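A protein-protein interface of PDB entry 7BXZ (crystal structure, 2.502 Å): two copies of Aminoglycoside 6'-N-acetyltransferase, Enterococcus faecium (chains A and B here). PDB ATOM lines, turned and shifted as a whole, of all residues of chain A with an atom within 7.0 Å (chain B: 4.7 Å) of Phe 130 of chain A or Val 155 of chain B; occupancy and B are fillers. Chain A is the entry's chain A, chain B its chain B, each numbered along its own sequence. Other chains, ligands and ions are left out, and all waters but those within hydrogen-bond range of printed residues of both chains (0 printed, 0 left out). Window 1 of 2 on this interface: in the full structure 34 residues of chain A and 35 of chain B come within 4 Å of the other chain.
The backbone NH (N) of Val 157 of chain A lies within hydrogen-bond range of the backbone carbonyl oxygen (O) of Val 155 of chain B (3.0 Å). O of Tyr 126 of chain A lies within hydrogen-bond range of NZ of Lys 153 of chain B (2.9 Å). The side-chain amino group (NZ) of Lys 153 of chain B lies within hydrogen-bond range of the side-chain hydroxyl (OG1) of Thr 129 of chain A (2.7 Å).
The backbone NH (N) of Val 155 of chain B lies within hydrogen-bond range of the backbone carbonyl oxygen (O) of Trp 170 of chain B (2.9 Å). O of Leu 125 of chain A lies within hydrogen-bond range of OG1 of Thr 129 of chain A, 2.5 Å away. N of Val 155 of chain A is in hydrogen-bond range of O of Trp 170 of chain A (2.9 Å). O of Gly 156 of chain A is in hydrogen-bond range of N of Trp 170 of chain A (2.8 Å). O of Gly 156 of chain B lies within hydrogen-bond range of N of Trp 170 of chain B. N of Ala 172 of chain B sits at hydrogen-bond distance from O of Lys 153 of chain B (2.9 Å).
Among the printed residues, merely in contact across the chains: Gly 156 of chain A with Val 155 of chain B (3.2 Å), Trp 170 of chain A with Trp 170 of chain B (3.2 Å), Val 155 of chain A with Gly 156 of chain B (3.2 Å), Phe 130 of chain A with Phe 130 of chain B (3.4 Å), Ile 154 of chain A with Phe 130 of chain B (3.5 Å), Phe 130 of chain A with Val 133 of chain B (3.6 Å), Tyr 126 of chain A with Ala 172 of chain B (3.6 Å), Val 133 of chain A with Phe 130 of chain B (3.6 Å), Gly 156 of chain A with Gly 156 of chain B (3.7 Å), Leu 158 of chain A with Ala 172 of chain B (3.8 Å), Phe 130 of chain A with Ile 154 of chain B (3.9 Å) and Phe 130 of chain A with Val 155 of chain B (3.9 Å).
Of the printed residues of chain B, Tyr 126 of chain A touches Lys 153 (2.9 Å) and Ala 172 (3.6 Å). Of the printed residues of chain B, Thr 129 of chain A touches Lys 153 (2.7 Å). Of the printed residues of chain B, Phe 130 of chain A touches Phe 130 (3.4 Å), Val 133 (3.6 Å), Ile 154 (3.9 Å) and Val 155 (3.9 Å). Ser 135 of chain A touches none of the printed residues of chain B. Printed residues of chain A within 4 Å of Phe 130 of chain B: Phe 130, Val 133 and Ile 154. Of the printed residues of chain A, Val 155 of chain B touches Phe 130, Gly 156 and Val 157. The nearest printed residue of chain B that does not touch Phe 130 of chain A is Gly 156 of chain B (4.002 Å). The nearest printed residue of chain A that does not touch Val 155 of chain B is Tyr 126 of chain A (4.001 Å). The nearest printed residue of chain A that does not touch Gly 156 of chain B is Phe 130 of chain A (4.002 Å).
Of the 18 printed residues of chain A, 10 touch a printed residue of chain B. Printed residues of chain A that touch a printed residue of chain B: Tyr 126, Thr 129, Phe 130, Val 133, Ile 154, Val 155, Gly 156, Val 157, Leu 158 and Trp 170. Of the 9 printed residues of chain B, 8 touch a printed residue of chain A. Hydrophobic or aromatic side chains of chain B that line the printed part of chain A: Phe 130, Val 133, Val 155, Trp 170 and Ala 172. Among the printed residues, no Asp or Glu carboxylate lies within 4 Å of a Lys or Arg side-chain nitrogen of the other chain.
Phe 130 of chain A touches Val 133 of chain B, and with the chains exchanged Val 133 of chain A touches Phe 130 of chain B. Phe 130 of chain A touches Ile 154 of chain B, and with the chains exchanged Ile 154 of chain A touches Phe 130 of chain B. Gly 156 of chain B touches its own counterpart, Gly 156 of chain A. Trp 170 of chain B touches its own counterpart, Trp 170 of chain A. 6 positions are printed for both chains.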
ATOM      1  N   LEU A 125      10.356  -6.707   5.019  1.00  0.00           N
ATOM      2  CA  LEU A 125      10.538  -8.117   4.702  1.00  0.00           C
ATOM      3  C   LEU A 125       9.604  -9.043   5.471  1.00  0.00           C
ATOM      4  O   LEU A 125       9.574 -10.239   5.169  1.00  0.00           O
ATOM      5  CB  LEU A 125      11.991  -8.519   4.949  1.00  0.00           C
ATOM      6  CG  LEU A 125      12.915  -8.248   3.762  1.00  0.00           C
ATOM      7  CD1 LEU A 125      14.364  -8.497   4.134  1.00  0.00           C
ATOM      8  CD2 LEU A 125      12.506  -9.098   2.568  1.00  0.00           C
ATOM      9  N   TYR A 126       8.855  -8.543   6.455  1.00  0.00           N
ATOM     10  CA  TYR A 126       7.862  -9.389   7.106  1.00  0.00           C
ATOM     11  C   TYR A 126       6.582  -9.537   6.293  1.00  0.00           C
ATOM     12  O   TYR A 126       5.760 -10.399   6.619  1.00  0.00           O
ATOM     13  CB  TYR A 126       7.522  -8.844   8.495  1.00  0.00           C
ATOM     14  CG  TYR A 126       8.637  -8.994   9.506  1.00  0.00           C
ATOM     15  CD1 TYR A 126       9.050 -10.251   9.931  1.00  0.00           C
ATOM     16  CD2 TYR A 126       9.273  -7.879  10.036  1.00  0.00           C
ATOM     17  CE1 TYR A 126      10.072 -10.393  10.857  1.00  0.00           C
ATOM     18  CE2 TYR A 126      10.293  -8.011  10.960  1.00  0.00           C
ATOM     19  CZ  TYR A 126      10.688  -9.270  11.367  1.00  0.00           C
ATOM     20  OH  TYR A 126      11.704  -9.404  12.286  1.00  0.00           O
ATOM     21  N   VAL A 127       6.400  -8.735   5.248  1.00  0.00           N
ATOM     22  CA  VAL A 127       5.243  -8.832   4.365  1.00  0.00           C
ATOM     23  C   VAL A 127       5.665  -9.583   3.110  1.00  0.00           C
ATOM     24  O   VAL A 127       6.495  -9.091   2.335  1.00  0.00           O
ATOM     25  CB  VAL A 127       4.685  -7.444   4.015  1.00  0.00           C
ATOM     26  CG1 VAL A 127       3.490  -7.576   3.081  1.00  0.00           C
ATOM     27  CG2 VAL A 127       4.306  -6.687   5.280  1.00  0.00           C
ATOM     28  N   HIS A 128       5.082 -10.763   2.902  1.00  0.00           N
ATOM     29  CA  HIS A 128       5.403 -11.624   1.763  1.00  0.00           C
ATOM     30  C   HIS A 128       6.910 -11.861   1.670  1.00  0.00           C
ATOM     31  O   HIS A 128       7.558 -11.575   0.663  1.00  0.00           O
ATOM     32  CB  HIS A 128       4.856 -11.037   0.460  1.00  0.00           C
ATOM     33  CG  HIS A 128       3.375 -10.822   0.471  1.00  0.00           C
ATOM     34  ND1 HIS A 128       2.805  -9.571   0.369  1.00  0.00           N
ATOM     35  CD2 HIS A 128       2.347 -11.698   0.574  1.00  0.00           C
ATOM     36  CE1 HIS A 128       1.489  -9.686   0.406  1.00  0.00           C
ATOM     37  NE2 HIS A 128       1.186 -10.965   0.531  1.00  0.00           N
ATOM     38  N   THR A 129       7.459 -12.380   2.771  1.00  0.00           N
ATOM     39  CA  THR A 129       8.903 -12.555   2.897  1.00  0.00           C
ATOM     40  C   THR A 129       9.461 -13.384   1.748  1.00  0.00           C
ATOM     41  O   THR A 129      10.357 -12.946   1.016  1.00  0.00           O
ATOM     42  CB  THR A 129       9.224 -13.222   4.236  1.00  0.00           C
ATOM     43  OG1 THR A 129       8.538 -12.539   5.293  1.00  0.00           O
ATOM     44  CG2 THR A 129      10.720 -13.198   4.501  1.00  0.00           C
ATOM     45  N   PHE A 130       8.937 -14.594   1.580  1.00  0.00           N
ATOM     46  CA  PHE A 130       9.516 -15.538   0.635  1.00  0.00           C
ATOM     47  C   PHE A 130       9.173 -15.198  -0.810  1.00  0.00           C
ATOM     48  O   PHE A 130       9.926 -15.566  -1.718  1.00  0.00           O
ATOM     49  CB  PHE A 130       9.102 -16.950   1.033  1.00  0.00           C
ATOM     50  CG  PHE A 130       9.662 -17.358   2.368  1.00  0.00           C
ATOM     51  CD1 PHE A 130      11.029 -17.295   2.593  1.00  0.00           C
ATOM     52  CD2 PHE A 130       8.835 -17.738   3.410  1.00  0.00           C
ATOM     53  CE1 PHE A 130      11.565 -17.641   3.817  1.00  0.00           C
ATOM     54  CE2 PHE A 130       9.367 -18.084   4.642  1.00  0.00           C
ATOM     55  CZ  PHE A 130      10.735 -18.035   4.843  1.00  0.00           C
ATOM     56  N   ASP A 131       8.065 -14.489  -1.048  1.00  0.00           N
ATOM     57  CA  ASP A 131       7.798 -14.013  -2.402  1.00  0.00           C
ATOM     58  C   ASP A 131       8.819 -12.960  -2.807  1.00  0.00           C
ATOM     59  O   ASP A 131       9.253 -12.916  -3.964  1.00  0.00           O
ATOM     60  CB  ASP A 131       6.386 -13.433  -2.503  1.00  0.00           C
ATOM     61  CG  ASP A 131       5.311 -14.498  -2.536  1.00  0.00           C
ATOM     62  OD1 ASP A 131       5.647 -15.688  -2.710  1.00  0.00           O
ATOM     63  OD2 ASP A 131       4.123 -14.140  -2.388  1.00  0.00           O
ATOM     64  N   LYS A 132       9.221 -12.110  -1.860  1.00  0.00           N
ATOM     65  CA  LYS A 132      10.268 -11.131  -2.134  1.00  0.00           C
ATOM     66  C   LYS A 132      11.633 -11.798  -2.254  1.00  0.00           C
ATOM     67  O   LYS A 132      12.479 -11.352  -3.039  1.00  0.00           O
ATOM     68  CB  LYS A 132      10.278 -10.062  -1.043  1.00  0.00           C
ATOM     69  CG  LYS A 132       9.058  -9.158  -1.066  1.00  0.00           C
ATOM     70  CD  LYS A 132       8.949  -8.322   0.197  1.00  0.00           C
ATOM     71  CE  LYS A 132       7.834  -7.296   0.080  1.00  0.00           C
ATOM     72  NZ  LYS A 132       7.886  -6.291   1.177  1.00  0.00           N
ATOM     73  N   VAL A 133      11.868 -12.862  -1.482  1.00  0.00           N
ATOM     74  CA  VAL A 133      13.137 -13.579  -1.580  1.00  0.00           C
ATOM     75  C   VAL A 133      13.261 -14.246  -2.945  1.00  0.00           C
ATOM     76  O   VAL A 133      14.306 -14.170  -3.602  1.00  0.00           O
ATOM     77  CB  VAL A 133      13.266 -14.600  -0.434  1.00  0.00           C
ATOM     78  CG1 VAL A 133      14.244 -15.707  -0.806  1.00  0.00           C
ATOM     79  CG2 VAL A 133      13.702 -13.911   0.842  1.00  0.00           C
ATOM     80  N   ALA A 134      12.187 -14.893  -3.399  1.00  0.00           N
ATOM     81  CA  ALA A 134      12.182 -15.558  -4.697  1.00  0.00           C
ATOM     82  C   ALA A 134      12.336 -14.581  -5.854  1.00  0.00           C
ATOM     83  O   ALA A 134      12.922 -14.943  -6.880  1.00  0.00           O
ATOM     84  CB  ALA A 134      10.892 -16.351  -4.870  1.00  0.00           C
ATOM     85  N   SER A 135      11.810 -13.362  -5.728  1.00  0.00           N
ATOM     86  CA  SER A 135      11.875 -12.381  -6.800  1.00  0.00           C
ATOM     87  C   SER A 135      13.038 -11.412  -6.644  1.00  0.00           C
ATOM     88  O   SER A 135      12.939 -10.274  -7.108  1.00  0.00           O
ATOM     89  CB  SER A 135      10.575 -11.586  -6.855  1.00  0.00           C
ATOM     90  OG  SER A 135       9.444 -12.432  -6.738  1.00  0.00           O
ATOM     91  N   ILE A 154      19.364 -18.704  -1.542  1.00  0.00           N
ATOM     92  CA  ILE A 154      18.862 -17.874  -0.455  1.00  0.00           C
ATOM     93  C   ILE A 154      17.777 -18.650   0.280  1.00  0.00           C
ATOM     94  O   ILE A 154      16.715 -18.942  -0.282  1.00  0.00           O
ATOM     95  CB  ILE A 154      18.331 -16.534  -0.979  1.00  0.00           C
ATOM     96  CG1 ILE A 154      19.447 -15.756  -1.678  1.00  0.00           C
ATOM     97  CG2 ILE A 154      17.754 -15.712   0.162  1.00  0.00           C
ATOM     98  CD1 ILE A 154      19.016 -14.386  -2.166  1.00  0.00           C
ATOM     99  N   VAL A 155      18.036 -18.980   1.543  1.00  0.00           N
ATOM    100  CA  VAL A 155      17.117 -19.776   2.343  1.00  0.00           C
ATOM    101  C   VAL A 155      16.545 -18.987   3.514  1.00  0.00           C
ATOM    102  O   VAL A 155      15.817 -19.552   4.335  1.00  0.00           O
ATOM    103  CB  VAL A 155      17.790 -21.067   2.836  1.00  0.00           C
ATOM    104  CG1 VAL A 155      18.111 -21.978   1.661  1.00  0.00           C
ATOM    105  CG2 VAL A 155      19.053 -20.738   3.619  1.00  0.00           C
ATOM    106  N   GLY A 156      16.833 -17.697   3.605  1.00  0.00           N
ATOM    107  CA  GLY A 156      16.311 -16.910   4.705  1.00  0.00           C
ATOM    108  C   GLY A 156      16.845 -15.496   4.666  1.00  0.00           C
ATOM    109  O   GLY A 156      17.827 -15.194   3.977  1.00  0.00           O
ATOM    110  N   VAL A 157      16.173 -14.629   5.425  1.00  0.00           N
ATOM    111  CA  VAL A 157      16.582 -13.241   5.597  1.00  0.00           C
ATOM    112  C   VAL A 157      16.342 -12.829   7.043  1.00  0.00           C
ATOM    113  O   VAL A 157      15.450 -13.349   7.718  1.00  0.00           O
ATOM    114  CB  VAL A 157      15.819 -12.291   4.648  1.00  0.00           C
ATOM    115  CG1 VAL A 157      16.295 -12.462   3.219  1.00  0.00           C
ATOM    116  CG2 VAL A 157      14.318 -12.535   4.751  1.00  0.00           C
ATOM    117  N   LEU A 158      17.158 -11.889   7.519  1.00  0.00           N
ATOM    118  CA  LEU A 158      16.986 -11.328   8.854  1.00  0.00           C
ATOM    119  C   LEU A 158      16.555  -9.875   8.712  1.00  0.00           C
ATOM    120  O   LEU A 158      17.399  -8.997   8.473  1.00  0.00           O
ATOM    121  CB  LEU A 158      18.272 -11.430   9.676  1.00  0.00           C
ATOM    122  CG  LEU A 158      18.116 -10.873  11.091  1.00  0.00           C
ATOM    123  CD1 LEU A 158      16.888 -11.467  11.759  1.00  0.00           C
ATOM    124  CD2 LEU A 158      19.355 -11.149  11.915  1.00  0.00           C
ATOM    125  N   PRO A 159      15.266  -9.570   8.850  1.00  0.00           N
ATOM    126  CA  PRO A 159      14.798  -8.201   8.600  1.00  0.00           C
ATOM    127  C   PRO A 159      15.387  -7.203   9.584  1.00  0.00           C
ATOM    128  O   PRO A 159      15.454  -7.453  10.790  1.00  0.00           O
ATOM    129  CB  PRO A 159      13.276  -8.313   8.763  1.00  0.00           C
ATOM    130  CG  PRO A 159      12.974  -9.780   8.635  1.00  0.00           C
ATOM    131  CD  PRO A 159      14.164 -10.482   9.194  1.00  0.00           C
ATOM    132  N   TRP A 170      20.607 -14.825   4.077  1.00  0.00           N
ATOM    133  CA  TRP A 170      21.164 -16.111   4.463  1.00  0.00           C
ATOM    134  C   TRP A 170      21.122 -17.047   3.269  1.00  0.00           C
ATOM    135  O   TRP A 170      20.061 -17.253   2.673  1.00  0.00           O
ATOM    136  CB  TRP A 170      20.382 -16.707   5.633  1.00  0.00           C
ATOM    137  CG  TRP A 170      20.671 -16.053   6.943  1.00  0.00           C
ATOM    138  CD1 TRP A 170      21.862 -15.533   7.354  1.00  0.00           C
ATOM    139  CD2 TRP A 170      19.749 -15.846   8.019  1.00  0.00           C
ATOM    140  NE1 TRP A 170      21.741 -15.017   8.622  1.00  0.00           N
ATOM    141  CE2 TRP A 170      20.453 -15.198   9.053  1.00  0.00           C
ATOM    142  CE3 TRP A 170      18.396 -16.143   8.207  1.00  0.00           C
ATOM    143  CZ2 TRP A 170      19.850 -14.845  10.257  1.00  0.00           C
ATOM    144  CZ3 TRP A 170      17.801 -15.797   9.404  1.00  0.00           C
ATOM    145  CH2 TRP A 170      18.527 -15.153  10.414  1.00  0.00           C
ATOM    146  N   PHE B 130       9.953 -22.865   0.388  1.00  0.00           N
ATOM    147  CA  PHE B 130       9.108 -21.853   1.010  1.00  0.00           C
ATOM    148  C   PHE B 130       7.653 -22.287   1.117  1.00  0.00           C
ATOM    149  O   PHE B 130       6.954 -21.852   2.038  1.00  0.00           O
ATOM    150  CB  PHE B 130       9.226 -20.542   0.236  1.00  0.00           C
ATOM    151  CG  PHE B 130      10.633 -20.033   0.140  1.00  0.00           C
ATOM    152  CD1 PHE B 130      11.557 -20.338   1.128  1.00  0.00           C
ATOM    153  CD2 PHE B 130      11.036 -19.258  -0.933  1.00  0.00           C
ATOM    154  CE1 PHE B 130      12.854 -19.879   1.052  1.00  0.00           C
ATOM    155  CE2 PHE B 130      12.337 -18.794  -1.015  1.00  0.00           C
ATOM    156  CZ  PHE B 130      13.247 -19.106  -0.022  1.00  0.00           C
ATOM    157  N   VAL B 133       7.682 -24.343   4.152  1.00  0.00           N
ATOM    158  CA  VAL B 133       7.770 -23.467   5.312  1.00  0.00           C
ATOM    159  C   VAL B 133       6.406 -22.858   5.611  1.00  0.00           C
ATOM    160  O   VAL B 133       5.974 -22.804   6.768  1.00  0.00           O
ATOM    161  CB  VAL B 133       8.839 -22.380   5.091  1.00  0.00           C
ATOM    162  CG1 VAL B 133       8.659 -21.254   6.097  1.00  0.00           C
ATOM    163  CG2 VAL B 133      10.232 -22.979   5.187  1.00  0.00           C
ATOM    164  N   LYS B 153       8.185 -14.738  13.617  1.00  0.00           N
ATOM    165  CA  LYS B 153       7.841 -15.320  12.328  1.00  0.00           C
ATOM    166  C   LYS B 153       9.025 -16.104  11.780  1.00  0.00           C
ATOM    167  O   LYS B 153      10.178 -15.693  11.935  1.00  0.00           O
ATOM    168  CB  LYS B 153       7.425 -14.241  11.322  1.00  0.00           C
ATOM    169  CG  LYS B 153       7.081 -14.794   9.945  1.00  0.00           C
ATOM    170  CD  LYS B 153       6.848 -13.698   8.918  1.00  0.00           C
ATOM    171  CE  LYS B 153       6.427 -14.295   7.583  1.00  0.00           C
ATOM    172  NZ  LYS B 153       6.237 -13.259   6.532  1.00  0.00           N
ATOM    173  N   ILE B 154       8.737 -17.235  11.138  1.00  0.00           N
ATOM    174  CA  ILE B 154       9.778 -17.993  10.455  1.00  0.00           C
ATOM    175  C   ILE B 154      10.264 -17.182   9.262  1.00  0.00           C
ATOM    176  O   ILE B 154       9.504 -16.913   8.324  1.00  0.00           O
ATOM    177  CB  ILE B 154       9.259 -19.368  10.014  1.00  0.00           C
ATOM    178  CG1 ILE B 154       8.872 -20.210  11.229  1.00  0.00           C
ATOM    179  CG2 ILE B 154      10.308 -20.084   9.177  1.00  0.00           C
ATOM    180  CD1 ILE B 154       8.399 -21.602  10.874  1.00  0.00           C
ATOM    181  N   VAL B 155      11.531 -16.779   9.297  1.00  0.00           N
ATOM    182  CA  VAL B 155      12.129 -15.976   8.238  1.00  0.00           C
ATOM    183  C   VAL B 155      13.218 -16.742   7.504  1.00  0.00           C
ATOM    184  O   VAL B 155      13.903 -16.172   6.648  1.00  0.00           O
ATOM    185  CB  VAL B 155      12.674 -14.646   8.783  1.00  0.00           C
ATOM    186  CG1 VAL B 155      11.530 -13.726   9.192  1.00  0.00           C
ATOM    187  CG2 VAL B 155      13.607 -14.904   9.953  1.00  0.00           C
ATOM    188  N   GLY B 156      13.405 -18.018   7.824  1.00  0.00           N
ATOM    189  CA  GLY B 156      14.387 -18.834   7.144  1.00  0.00           C
ATOM    190  C   GLY B 156      14.535 -20.209   7.756  1.00  0.00           C
ATOM    191  O   GLY B 156      14.140 -20.431   8.903  1.00  0.00           O
ATOM    192  N   TRP B 170      14.789 -20.695  11.465  1.00  0.00           N
ATOM    193  CA  TRP B 170      15.196 -19.354  11.858  1.00  0.00           C
ATOM    194  C   TRP B 170      13.963 -18.471  11.997  1.00  0.00           C
ATOM    195  O   TRP B 170      13.152 -18.374  11.070  1.00  0.00           O
ATOM    196  CB  TRP B 170      16.183 -18.779  10.840  1.00  0.00           C
ATOM    197  CG  TRP B 170      17.547 -19.406  10.954  1.00  0.00           C
ATOM    198  CD1 TRP B 170      18.124 -19.896  12.089  1.00  0.00           C
ATOM    199  CD2 TRP B 170      18.496 -19.621   9.900  1.00  0.00           C
ATOM    200  NE1 TRP B 170      19.372 -20.394  11.811  1.00  0.00           N
ATOM    201  CE2 TRP B 170      19.625 -20.238  10.473  1.00  0.00           C
ATOM    202  CE3 TRP B 170      18.500 -19.353   8.528  1.00  0.00           C
ATOM    203  CZ2 TRP B 170      20.748 -20.586   9.724  1.00  0.00           C
ATOM    204  CZ3 TRP B 170      19.618 -19.696   7.786  1.00  0.00           C
ATOM    205  CH2 TRP B 170      20.725 -20.308   8.386  1.00  0.00           C
ATOM    206  N   MET B 171      13.823 -17.834  13.157  1.00  0.00           N
ATOM    207  CA  MET B 171      12.665 -17.011  13.466  1.00  0.00           C
ATOM    208  C   MET B 171      13.119 -15.622  13.882  1.00  0.00           C
ATOM    209  O   MET B 171      14.172 -15.459  14.498  1.00  0.00           O
ATOM    210  CB  MET B 171      11.825 -17.646  14.582  1.00  0.00           C
ATOM    211  CG  MET B 171      11.383 -19.067  14.280  1.00  0.00           C
ATOM    212  SD  MET B 171      10.221 -19.715  15.491  1.00  0.00           S
ATOM    213  CE  MET B 171       8.709 -18.921  14.956  1.00  0.00           C
ATOM    214  N   ALA B 172      12.325 -14.615  13.526  1.00  0.00           N
ATOM    215  CA  ALA B 172      12.677 -13.233  13.817  1.00  0.00           C
ATOM    216  C   ALA B 172      11.442 -12.439  14.216  1.00  0.00           C
ATOM    217  O   ALA B 172      10.314 -12.776  13.845  1.00  0.00           O
ATOM    218  CB  ALA B 172      13.355 -12.552  12.620  1.00  0.00           C
